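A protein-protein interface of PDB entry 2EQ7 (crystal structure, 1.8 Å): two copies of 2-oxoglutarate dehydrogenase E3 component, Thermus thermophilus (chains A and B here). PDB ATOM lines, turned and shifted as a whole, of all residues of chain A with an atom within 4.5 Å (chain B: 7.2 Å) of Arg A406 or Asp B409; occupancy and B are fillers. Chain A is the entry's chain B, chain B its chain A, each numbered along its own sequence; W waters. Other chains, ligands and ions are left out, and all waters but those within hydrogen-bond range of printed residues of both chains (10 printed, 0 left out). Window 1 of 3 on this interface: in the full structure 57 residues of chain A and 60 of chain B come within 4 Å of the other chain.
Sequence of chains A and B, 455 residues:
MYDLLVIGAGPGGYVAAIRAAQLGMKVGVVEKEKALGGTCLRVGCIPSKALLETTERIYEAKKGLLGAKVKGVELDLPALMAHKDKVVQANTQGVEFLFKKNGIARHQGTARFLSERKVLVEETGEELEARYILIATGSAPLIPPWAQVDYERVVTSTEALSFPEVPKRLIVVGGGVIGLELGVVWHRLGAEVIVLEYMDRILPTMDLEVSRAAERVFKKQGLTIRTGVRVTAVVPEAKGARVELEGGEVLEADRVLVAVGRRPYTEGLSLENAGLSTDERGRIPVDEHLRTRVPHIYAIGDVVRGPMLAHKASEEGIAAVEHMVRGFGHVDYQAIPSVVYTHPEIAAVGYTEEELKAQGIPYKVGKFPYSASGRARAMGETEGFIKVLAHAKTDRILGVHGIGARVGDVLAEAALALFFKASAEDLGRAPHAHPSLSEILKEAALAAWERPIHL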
ATOM      1  N   GLU A 345      22.049  -8.787 -19.649  1.00  0.00           N
ATOM      2  CA  GLU A 345      21.167  -8.532 -20.780  1.00  0.00           C
ATOM      3  C   GLU A 345      22.062  -8.532 -22.013  1.00  0.00           C
ATOM      4  O   GLU A 345      23.282  -8.428 -21.896  1.00  0.00           O
ATOM      5  CB  GLU A 345      20.462  -7.170 -20.648  1.00  0.00           C
ATOM      6  CG  GLU A 345      19.544  -7.050 -19.437  1.00  0.00           C
ATOM      7  CD  GLU A 345      18.588  -5.869 -19.515  1.00  0.00           C
ATOM      8  OE1 GLU A 345      18.893  -4.875 -20.218  1.00  0.00           O
ATOM      9  OE2 GLU A 345      17.526  -5.929 -18.857  1.00  0.00           O
ATOM     10  N   TYR A 370      32.876  -3.907 -19.000  1.00  0.00           N
ATOM     11  CA  TYR A 370      32.214  -3.636 -17.730  1.00  0.00           C
ATOM     12  C   TYR A 370      33.240  -3.724 -16.605  1.00  0.00           C
ATOM     13  O   TYR A 370      33.070  -3.119 -15.546  1.00  0.00           O
ATOM     14  CB  TYR A 370      31.113  -4.659 -17.473  1.00  0.00           C
ATOM     15  CG  TYR A 370      29.742  -4.236 -17.940  1.00  0.00           C
ATOM     16  CD1 TYR A 370      28.703  -4.068 -17.024  1.00  0.00           C
ATOM     17  CD2 TYR A 370      29.471  -4.026 -19.294  1.00  0.00           C
ATOM     18  CE1 TYR A 370      27.424  -3.706 -17.441  1.00  0.00           C
ATOM     19  CE2 TYR A 370      28.194  -3.663 -19.723  1.00  0.00           C
ATOM     20  CZ  TYR A 370      27.177  -3.509 -18.789  1.00  0.00           C
ATOM     21  OH  TYR A 370      25.903  -3.187 -19.199  1.00  0.00           O
ATOM     22  N   MET A 379      28.591  -2.711  -8.126  1.00  0.00           N
ATOM     23  CA  MET A 379      27.457  -3.636  -8.149  1.00  0.00           C
ATOM     24  C   MET A 379      27.900  -5.084  -7.982  1.00  0.00           C
ATOM     25  O   MET A 379      27.095  -5.953  -7.649  1.00  0.00           O
ATOM     26  CB  MET A 379      26.714  -3.545  -9.482  1.00  0.00           C
ATOM     27  CG  MET A 379      26.043  -2.234  -9.774  1.00  0.00           C
ATOM     28  SD  MET A 379      25.542  -2.250 -11.507  1.00  0.00           S
ATOM     29  CE  MET A 379      24.199  -3.434 -11.455  1.00  0.00           C
ATOM     30  N   GLY A 404      25.828  -7.342 -20.829  1.00  0.00           N
ATOM     31  CA  GLY A 404      26.164  -6.935 -19.476  1.00  0.00           C
ATOM     32  C   GLY A 404      24.929  -6.565 -18.682  1.00  0.00           C
ATOM     33  O   GLY A 404      23.838  -6.439 -19.241  1.00  0.00           O
ATOM     34  N   ALA A 405      25.096  -6.390 -17.375  1.00  0.00           N
ATOM     35  CA  ALA A 405      23.974  -6.032 -16.516  1.00  0.00           C
ATOM     36  C   ALA A 405      23.266  -4.789 -17.053  1.00  0.00           C
ATOM     37  O   ALA A 405      23.902  -3.771 -17.311  1.00  0.00           O
ATOM     38  CB  ALA A 405      24.465  -5.780 -15.086  1.00  0.00           C
ATOM     39  N   ARG A 406      21.953  -4.901 -17.240  1.00  0.00           N
ATOM     40  CA  ARG A 406      21.113  -3.805 -17.728  1.00  0.00           C
ATOM     41  C   ARG A 406      21.612  -3.116 -18.996  1.00  0.00           C
ATOM     42  O   ARG A 406      21.349  -1.936 -19.205  1.00  0.00           O
ATOM     43  CB  ARG A 406      20.946  -2.769 -16.618  1.00  0.00           C
ATOM     44  CG  ARG A 406      20.421  -3.378 -15.331  1.00  0.00           C
ATOM     45  CD  ARG A 406      20.454  -2.393 -14.190  1.00  0.00           C
ATOM     46  NE  ARG A 406      20.317  -3.078 -12.910  1.00  0.00           N
ATOM     47  CZ  ARG A 406      20.419  -2.478 -11.732  1.00  0.00           C
ATOM     48  NH1 ARG A 406      20.657  -1.176 -11.670  1.00  0.00           N
ATOM     49  NH2 ARG A 406      20.293  -3.184 -10.617  1.00  0.00           N
ATOM     50  N   VAL A 407      22.304  -3.851 -19.858  1.00  0.00           N
ATOM     51  CA  VAL A 407      22.835  -3.240 -21.071  1.00  0.00           C
ATOM     52  C   VAL A 407      21.723  -2.720 -21.977  1.00  0.00           C
ATOM     53  O   VAL A 407      21.927  -1.781 -22.744  1.00  0.00           O
ATOM     54  CB  VAL A 407      23.752  -4.226 -21.844  1.00  0.00           C
ATOM     55  CG1 VAL A 407      22.935  -5.125 -22.750  1.00  0.00           C
ATOM     56  CG2 VAL A 407      24.808  -3.444 -22.628  1.00  0.00           C
ATOM     57  N   GLY A 408      20.544  -3.326 -21.874  1.00  0.00           N
ATOM     58  CA  GLY A 408      19.415  -2.887 -22.674  1.00  0.00           C
ATOM     59  C   GLY A 408      18.999  -1.485 -22.267  1.00  0.00           C
ATOM     60  O   GLY A 408      18.657  -0.659 -23.117  1.00  0.00           O
ATOM     61  N   ASP A 409      19.014  -1.214 -20.964  1.00  0.00           N
ATOM     62  CA  ASP A 409      18.651   0.108 -20.466  1.00  0.00           C
ATOM     63  C   ASP A 409      19.701   1.110 -20.914  1.00  0.00           C
ATOM     64  O   ASP A 409      19.382   2.242 -21.281  1.00  0.00           O
ATOM     65  CB  ASP A 409      18.562   0.117 -18.938  1.00  0.00           C
ATOM     66  CG  ASP A 409      17.454  -0.772 -18.414  1.00  0.00           C
ATOM     67  OD1 ASP A 409      16.414  -0.890 -19.095  1.00  0.00           O
ATOM     68  OD2 ASP A 409      17.614  -1.339 -17.314  1.00  0.00           O
ATOM     69  N   VAL A 410      20.959   0.692 -20.887  1.00  0.00           N
ATOM     70  CA  VAL A 410      22.032   1.581 -21.305  1.00  0.00           C
ATOM     71  C   VAL A 410      21.877   1.938 -22.777  1.00  0.00           C
ATOM     72  O   VAL A 410      22.016   3.103 -23.159  1.00  0.00           O
ATOM     73  CB  VAL A 410      23.418   0.935 -21.092  1.00  0.00           C
ATOM     74  CG1 VAL A 410      24.512   1.856 -21.642  1.00  0.00           C
ATOM     75  CG2 VAL A 410      23.647   0.688 -19.604  1.00  0.00           C
ATOM     76  N   LEU A 437      26.302   3.049 -15.329  1.00  0.00           N
ATOM     77  CA  LEU A 437      26.622   2.130 -16.410  1.00  0.00           C
ATOM     78  C   LEU A 437      26.619   2.847 -17.757  1.00  0.00           C
ATOM     79  O   LEU A 437      27.232   2.377 -18.713  1.00  0.00           O
ATOM     80  CB  LEU A 437      25.643   0.952 -16.430  1.00  0.00           C
ATOM     81  CG  LEU A 437      25.675   0.037 -15.198  1.00  0.00           C
ATOM     82  CD1 LEU A 437      24.630  -1.059 -15.355  1.00  0.00           C
ATOM     83  CD2 LEU A 437      27.070  -0.571 -15.025  1.00  0.00           C
ATOM     84  N   GLU B  53      24.371  -0.219  -3.560  1.00  0.00           N
ATOM     85  CA  GLU B  53      24.006  -1.347  -4.414  1.00  0.00           C
ATOM     86  C   GLU B  53      23.855  -2.642  -3.617  1.00  0.00           C
ATOM     87  O   GLU B  53      22.861  -3.363  -3.753  1.00  0.00           O
ATOM     88  CB  GLU B  53      25.059  -1.554  -5.509  1.00  0.00           C
ATOM     89  CG  GLU B  53      25.099  -0.467  -6.582  1.00  0.00           C
ATOM     90  CD  GLU B  53      23.907  -0.507  -7.534  1.00  0.00           C
ATOM     91  OE1 GLU B  53      23.885   0.303  -8.487  1.00  0.00           O
ATOM     92  OE2 GLU B  53      22.994  -1.338  -7.339  1.00  0.00           O
ATOM     93  N   ARG B  57      20.179  -4.999  -2.162  1.00  0.00           N
ATOM     94  CA  ARG B  57      19.876  -6.408  -2.413  1.00  0.00           C
ATOM     95  C   ARG B  57      19.598  -7.142  -1.106  1.00  0.00           C
ATOM     96  O   ARG B  57      18.713  -7.994  -1.038  1.00  0.00           O
ATOM     97  CB  ARG B  57      21.036  -7.084  -3.150  1.00  0.00           C
ATOM     98  CG  ARG B  57      21.351  -6.454  -4.490  1.00  0.00           C
ATOM     99  CD  ARG B  57      20.151  -6.520  -5.423  1.00  0.00           C
ATOM    100  NE  ARG B  57      20.267  -5.562  -6.518  1.00  0.00           N
ATOM    101  CZ  ARG B  57      19.417  -5.479  -7.537  1.00  0.00           C
ATOM    102  NH1 ARG B  57      18.381  -6.304  -7.610  1.00  0.00           N
ATOM    103  NH2 ARG B  57      19.601  -4.566  -8.482  1.00  0.00           N
ATOM    104  N   VAL B 339      21.859  12.705  -9.768  1.00  0.00           N
ATOM    105  CA  VAL B 339      21.158  11.501  -9.341  1.00  0.00           C
ATOM    106  C   VAL B 339      21.391  11.124  -7.881  1.00  0.00           C
ATOM    107  O   VAL B 339      22.500  11.263  -7.363  1.00  0.00           O
ATOM    108  CB  VAL B 339      21.577  10.296 -10.218  1.00  0.00           C
ATOM    109  CG1 VAL B 339      20.706   9.093  -9.905  1.00  0.00           C
ATOM    110  CG2 VAL B 339      21.483  10.663 -11.700  1.00  0.00           C
ATOM    111  N   TYR B 341      21.277   7.966  -5.490  1.00  0.00           N
ATOM    112  CA  TYR B 341      21.303   6.522  -5.669  1.00  0.00           C
ATOM    113  C   TYR B 341      20.644   5.622  -4.644  1.00  0.00           C
ATOM    114  O   TYR B 341      21.137   4.540  -4.330  1.00  0.00           O
ATOM    115  CB  TYR B 341      22.742   6.078  -5.930  1.00  0.00           C
ATOM    116  CG  TYR B 341      23.271   6.662  -7.224  1.00  0.00           C
ATOM    117  CD1 TYR B 341      24.120   7.765  -7.226  1.00  0.00           C
ATOM    118  CD2 TYR B 341      22.865   6.142  -8.454  1.00  0.00           C
ATOM    119  CE1 TYR B 341      24.554   8.338  -8.429  1.00  0.00           C
ATOM    120  CE2 TYR B 341      23.287   6.704  -9.654  1.00  0.00           C
ATOM    121  CZ  TYR B 341      24.130   7.799  -9.636  1.00  0.00           C
ATOM    122  OH  TYR B 341      24.538   8.355 -10.829  1.00  0.00           O
ATOM    123  N   GLU B 345      15.543   5.407  -7.179  1.00  0.00           N
ATOM    124  CA  GLU B 345      16.534   6.440  -7.445  1.00  0.00           C
ATOM    125  C   GLU B 345      15.753   7.735  -7.641  1.00  0.00           C
ATOM    126  O   GLU B 345      14.531   7.716  -7.821  1.00  0.00           O
ATOM    127  CB  GLU B 345      17.351   6.126  -8.708  1.00  0.00           C
ATOM    128  CG  GLU B 345      18.188   4.852  -8.614  1.00  0.00           C
ATOM    129  CD  GLU B 345      19.230   4.726  -9.720  1.00  0.00           C
ATOM    130  OE1 GLU B 345      19.031   5.295 -10.821  1.00  0.00           O
ATOM    131  OE2 GLU B 345      20.247   4.038  -9.491  1.00  0.00           O
ATOM    132  N   ALA B 347      16.234  11.598  -9.689  1.00  0.00           N
ATOM    133  CA  ALA B 347      17.095  12.297 -10.633  1.00  0.00           C
ATOM    134  C   ALA B 347      16.527  13.585 -11.204  1.00  0.00           C
ATOM    135  O   ALA B 347      15.312  13.804 -11.224  1.00  0.00           O
ATOM    136  CB  ALA B 347      17.479  11.351 -11.773  1.00  0.00           C
ATOM    137  N   ARG B 375       6.899  -2.864 -17.780  1.00  0.00           N
ATOM    138  CA  ARG B 375       8.180  -3.353 -17.282  1.00  0.00           C
ATOM    139  C   ARG B 375       8.266  -3.150 -15.774  1.00  0.00           C
ATOM    140  O   ARG B 375       8.743  -4.022 -15.048  1.00  0.00           O
ATOM    141  CB  ARG B 375       9.343  -2.625 -17.969  1.00  0.00           C
ATOM    142  CG  ARG B 375      10.734  -3.089 -17.516  1.00  0.00           C
ATOM    143  CD  ARG B 375      10.953  -4.582 -17.775  1.00  0.00           C
ATOM    144  NE  ARG B 375      12.327  -4.976 -17.465  1.00  0.00           N
ATOM    145  CZ  ARG B 375      13.368  -4.744 -18.259  1.00  0.00           C
ATOM    146  NH1 ARG B 375      14.586  -5.125 -17.891  1.00  0.00           N
ATOM    147  NH2 ARG B 375      13.190  -4.153 -19.435  1.00  0.00           N
ATOM    148  N   ALA B 405      12.516   3.194  -9.665  1.00  0.00           N
ATOM    149  CA  ALA B 405      13.579   2.219  -9.879  1.00  0.00           C
ATOM    150  C   ALA B 405      14.456   2.586 -11.079  1.00  0.00           C
ATOM    151  O   ALA B 405      13.955   2.840 -12.170  1.00  0.00           O
ATOM    152  CB  ALA B 405      12.973   0.824 -10.077  1.00  0.00           C
ATOM    153  N   ARG B 406      15.767   2.631 -10.851  1.00  0.00           N
ATOM    154  CA  ARG B 406      16.746   2.944 -11.893  1.00  0.00           C
ATOM    155  C   ARG B 406      16.415   4.179 -12.727  1.00  0.00           C
ATOM    156  O   ARG B 406      16.802   4.266 -13.892  1.00  0.00           O
ATOM    157  CB  ARG B 406      16.902   1.735 -12.810  1.00  0.00           C
ATOM    158  CG  ARG B 406      17.202   0.459 -12.040  1.00  0.00           C
ATOM    159  CD  ARG B 406      17.126  -0.763 -12.925  1.00  0.00           C
ATOM    160  NE  ARG B 406      17.047  -1.983 -12.127  1.00  0.00           N
ATOM    161  CZ  ARG B 406      16.815  -3.188 -12.634  1.00  0.00           C
ATOM    162  NH1 ARG B 406      16.641  -3.332 -13.940  1.00  0.00           N
ATOM    163  NH2 ARG B 406      16.747  -4.242 -11.834  1.00  0.00           N
ATOM    164  N   VAL B 407      15.730   5.151 -12.134  1.00  0.00           N
ATOM    165  CA  VAL B 407      15.366   6.342 -12.890  1.00  0.00           C
ATOM    166  C   VAL B 407      16.603   7.097 -13.378  1.00  0.00           C
ATOM    167  O   VAL B 407      16.557   7.779 -14.402  1.00  0.00           O
ATOM    168  CB  VAL B 407      14.445   7.278 -12.061  1.00  0.00           C
ATOM    169  CG1 VAL B 407      15.261   8.159 -11.131  1.00  0.00           C
ATOM    170  CG2 VAL B 407      13.580   8.112 -13.005  1.00  0.00           C
ATOM    171  N   GLY B 408      17.708   6.962 -12.652  1.00  0.00           N
ATOM    172  CA  GLY B 408      18.937   7.623 -13.054  1.00  0.00           C
ATOM    173  C   GLY B 408      19.424   7.062 -14.377  1.00  0.00           C
ATOM    174  O   GLY B 408      19.917   7.798 -15.235  1.00  0.00           O
ATOM    175  N   ASP B 409      19.298   5.749 -14.544  1.00  0.00           N
ATOM    176  CA  ASP B 409      19.714   5.110 -15.782  1.00  0.00           C
ATOM    177  C   ASP B 409      18.808   5.565 -16.915  1.00  0.00           C
ATOM    178  O   ASP B 409      19.265   5.825 -18.027  1.00  0.00           O
ATOM    179  CB  ASP B 409      19.645   3.586 -15.664  1.00  0.00           C
ATOM    180  CG  ASP B 409      20.642   3.034 -14.670  1.00  0.00           C
ATOM    181  OD1 ASP B 409      21.714   3.650 -14.497  1.00  0.00           O
ATOM    182  OD2 ASP B 409      20.362   1.974 -14.075  1.00  0.00           O
ATOM    183  N   VAL B 410      17.516   5.664 -16.628  1.00  0.00           N
ATOM    184  CA  VAL B 410      16.567   6.091 -17.645  1.00  0.00           C
ATOM    185  C   VAL B 410      16.864   7.512 -18.113  1.00  0.00           C
ATOM    186  O   VAL B 410      16.789   7.803 -19.308  1.00  0.00           O
ATOM    187  CB  VAL B 410      15.115   6.034 -17.120  1.00  0.00           C
ATOM    188  CG1 VAL B 410      14.156   6.586 -18.173  1.00  0.00           C
ATOM    189  CG2 VAL B 410      14.742   4.592 -16.789  1.00  0.00           C
ATOM    190  N   LEU B 411      17.217   8.389 -17.175  1.00  0.00           N
ATOM    191  CA  LEU B 411      17.494   9.775 -17.520  1.00  0.00           C
ATOM    192  C   LEU B 411      18.824  10.034 -18.215  1.00  0.00           C
ATOM    193  O   LEU B 411      19.136  11.175 -18.561  1.00  0.00           O
ATOM    194  CB  LEU B 411      17.328  10.672 -16.282  1.00  0.00           C
ATOM    195  CG  LEU B 411      15.940  11.338 -16.199  1.00  0.00           C
ATOM    196  CD1 LEU B 411      14.832  10.306 -16.409  1.00  0.00           C
ATOM    197  CD2 LEU B 411      15.776  12.043 -14.858  1.00  0.00           C
ATOM    198  N   ALA B 412      19.611   8.984 -18.428  1.00  0.00           N
ATOM    199  CA  ALA B 412      20.869   9.154 -19.143  1.00  0.00           C
ATOM    200  C   ALA B 412      20.444   9.589 -20.546  1.00  0.00           C
ATOM    201  O   ALA B 412      21.106  10.394 -21.197  1.00  0.00           O
ATOM    202  CB  ALA B 412      21.633   7.833 -19.208  1.00  0.00           C
ATOM    203  N   GLU B 413      19.310   9.048 -20.988  1.00  0.00           N
ATOM    204  CA  GLU B 413      18.750   9.350 -22.300  1.00  0.00           C
ATOM    205  C   GLU B 413      18.252  10.797 -22.328  1.00  0.00           C
ATOM    206  O   GLU B 413      18.366  11.490 -23.343  1.00  0.00           O
ATOM    207  CB  GLU B 413      17.586   8.397 -22.592  1.00  0.00           C
ATOM    208  CG  GLU B 413      17.193   8.314 -24.048  1.00  0.00           C
ATOM    209  CD  GLU B 413      15.879   7.583 -24.261  1.00  0.00           C
ATOM    210  OE1 GLU B 413      15.643   6.549 -23.596  1.00  0.00           O
ATOM    211  OE2 GLU B 413      15.084   8.041 -25.104  1.00  0.00           O
ATOM    212  N   ALA B 414      17.696  11.247 -21.207  1.00  0.00           N
ATOM    213  CA  ALA B 414      17.186  12.608 -21.101  1.00  0.00           C
ATOM    214  C   ALA B 414      18.334  13.604 -21.225  1.00  0.00           C
ATOM    215  O   ALA B 414      18.193  14.656 -21.856  1.00  0.00           O
ATOM    216  CB  ALA B 414      16.467  12.799 -19.768  1.00  0.00           C
ATOM    217  N   LEU B 437      11.925   0.362 -18.960  1.00  0.00           N
ATOM    218  CA  LEU B 437      11.626   1.547 -18.166  1.00  0.00           C
ATOM    219  C   LEU B 437      11.805   2.808 -19.001  1.00  0.00           C
ATOM    220  O   LEU B 437      11.239   3.853 -18.679  1.00  0.00           O
ATOM    221  CB  LEU B 437      12.519   1.607 -16.923  1.00  0.00           C
ATOM    222  CG  LEU B 437      12.320   0.486 -15.894  1.00  0.00           C
ATOM    223  CD1 LEU B 437      13.277   0.699 -14.720  1.00  0.00           C
ATOM    224  CD2 LEU B 437      10.865   0.468 -15.407  1.00  0.00           C
ATOM    225  N   SER B 438      12.574   2.712 -20.083  1.00  0.00           N
ATOM    226  CA  SER B 438      12.796   3.877 -20.932  1.00  0.00           C
ATOM    227  C   SER B 438      11.481   4.360 -21.545  1.00  0.00           C
ATOM    228  O   SER B 438      11.352   5.527 -21.901  1.00  0.00           O
ATOM    229  CB  SER B 438      13.812   3.566 -22.042  1.00  0.00           C
ATOM    230  OG  SER B 438      13.272   2.703 -23.032  1.00  0.00           O
ATOM    231  N   LEU B 441       9.920   7.378 -19.930  1.00  0.00           N
ATOM    232  CA  LEU B 441      10.465   8.656 -20.379  1.00  0.00           C
ATOM    233  C   LEU B 441       9.837   9.031 -21.725  1.00  0.00           C
ATOM    234  O   LEU B 441       9.486  10.190 -21.965  1.00  0.00           O
ATOM    235  CB  LEU B 441      11.981   8.554 -20.533  1.00  0.00           C
ATOM    236  CG  LEU B 441      12.678   9.766 -21.149  1.00  0.00           C
ATOM    237  CD1 LEU B 441      12.478  10.993 -20.254  1.00  0.00           C
ATOM    238  CD2 LEU B 441      14.154   9.457 -21.330  1.00  0.00           C
HETATM  239  O   HOH W   1      19.407   5.384 -21.183  1.00  0.00           O
HETATM  240  O   HOH W   2      24.027   2.678 -13.620  1.00  0.00           O
HETATM  241  O   HOH W   3      14.014  -1.405 -18.231  1.00  0.00           O
HETATM  242  O   HOH W   4      17.352  -4.151 -16.759  1.00  0.00           O
HETATM  243  O   HOH W   5      18.854  -0.040 -15.342  1.00  0.00           O
HETATM  244  O   HOH W   6      23.555   0.128 -11.664  1.00  0.00           O
HETATM  245  O   HOH W   7      15.144   1.032 -20.456  1.00  0.00           O
HETATM  246  O   HOH W   8      20.866  -0.560  -9.191  1.00  0.00           O
HETATM  247  O   HOH W   9      20.459   1.781 -11.321  1.00  0.00           O
HETATM  248  O   HOH W  10      16.214  -3.417 -20.118  1.00  0.00           O
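The side-chain carboxylate (OE2) of Glu A345 is in salt-bridge range of the guanidinium group (NH1) of Arg B375, 3.2 Å away. The guanidinium group (NH1) of Arg A406 lies within salt-bridge range of the side-chain carboxylate (OD2) of Asp B409. The guanidinium group (NH2) of Arg B57 lies close to the guanidinium group (NH2) of Arg A406.
The side-chain carboxylate (OE1) of Glu A345 sits at hydrogen-bond distance from the backbone NH (N) of Gly A408 (2.8 Å). The backbone carbonyl oxygen of Glu A345 sits at hydrogen-bond distance from the backbone NH of Gly A404, at 3.0 Å.
Among the printed residues, merely in contact across the chains: Arg A406 with Arg B406 and Met A379 with Glu B53.
Of chain B, only Arg B57 (2.6 Å), Arg B406 (3.4 Å) and Asp B409 (3.97 Å) come within 4 Å of Arg A406. Printed residues of chain A within 4 Å of Asp B409: Arg A406 (3.97 Å). Of the printed residues of chain B, Met A379 touches Glu B53 (3.5 Å). Of the printed residues of chain B, Glu A345 touches Arg B375. The nearest residue of chain B that does not touch Arg A406 is Glu B53 (4.6 Å). The nearest printed residue of chain A that does not touch Asp B409 is Leu A437 (4.7 Å).
Printed residues of chain A that touch a printed residue of chain B: Glu A345, Met A379 and Arg A406. Hydrophobic or aromatic side chains of chain A that line the printed part of chain B: Met A379. Among the printed residues, 5 pairs touch across the chains.
Arg A406 touches its own counterpart, Arg B406. Arg A406 touches Asp B409, but with the chains exchanged Asp A409 does not touch Arg B406 (4.04 Å). Of the 5 pairs that touch across the chains among the printed residues, 1 has its exchanged pair printed and touching as well.
Water W8 bridges NH1 of Arg A406 (2.6 Å) and OE2 of Glu B53 (2.9 Å). Water W7 lies within hydrogen-bond range of OD1 of Asp A409 (2.7 Å) and N of Ser B438 (3.1 Å). Water W10 lies within hydrogen-bond range of the side-chain carboxylate (OD1) of Asp A409 (2.7 Å), the side-chain carboxylate (OE1) of Glu A345 (3.1 Å) and the guanidinium group (NH2) of Arg B375 (3.2 Å). Water W4 lies within hydrogen-bond range of OE2 of Glu A345, OD2 of Asp A409, NH1 of Arg B406 and NH1 of Arg B375. Water W6 lies within hydrogen-bond range of SD of Met A379 (3.1 Å), NH1 of Arg A406 (3.2 Å) and OE1 of Glu B53 (3.2 Å). Water W1 lies within hydrogen-bond range of the backbone carbonyl oxygen (O) of Asp A409 (3.1 Å) and the backbone carbonyl oxygen (O) of Asp B409 (3.2 Å).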
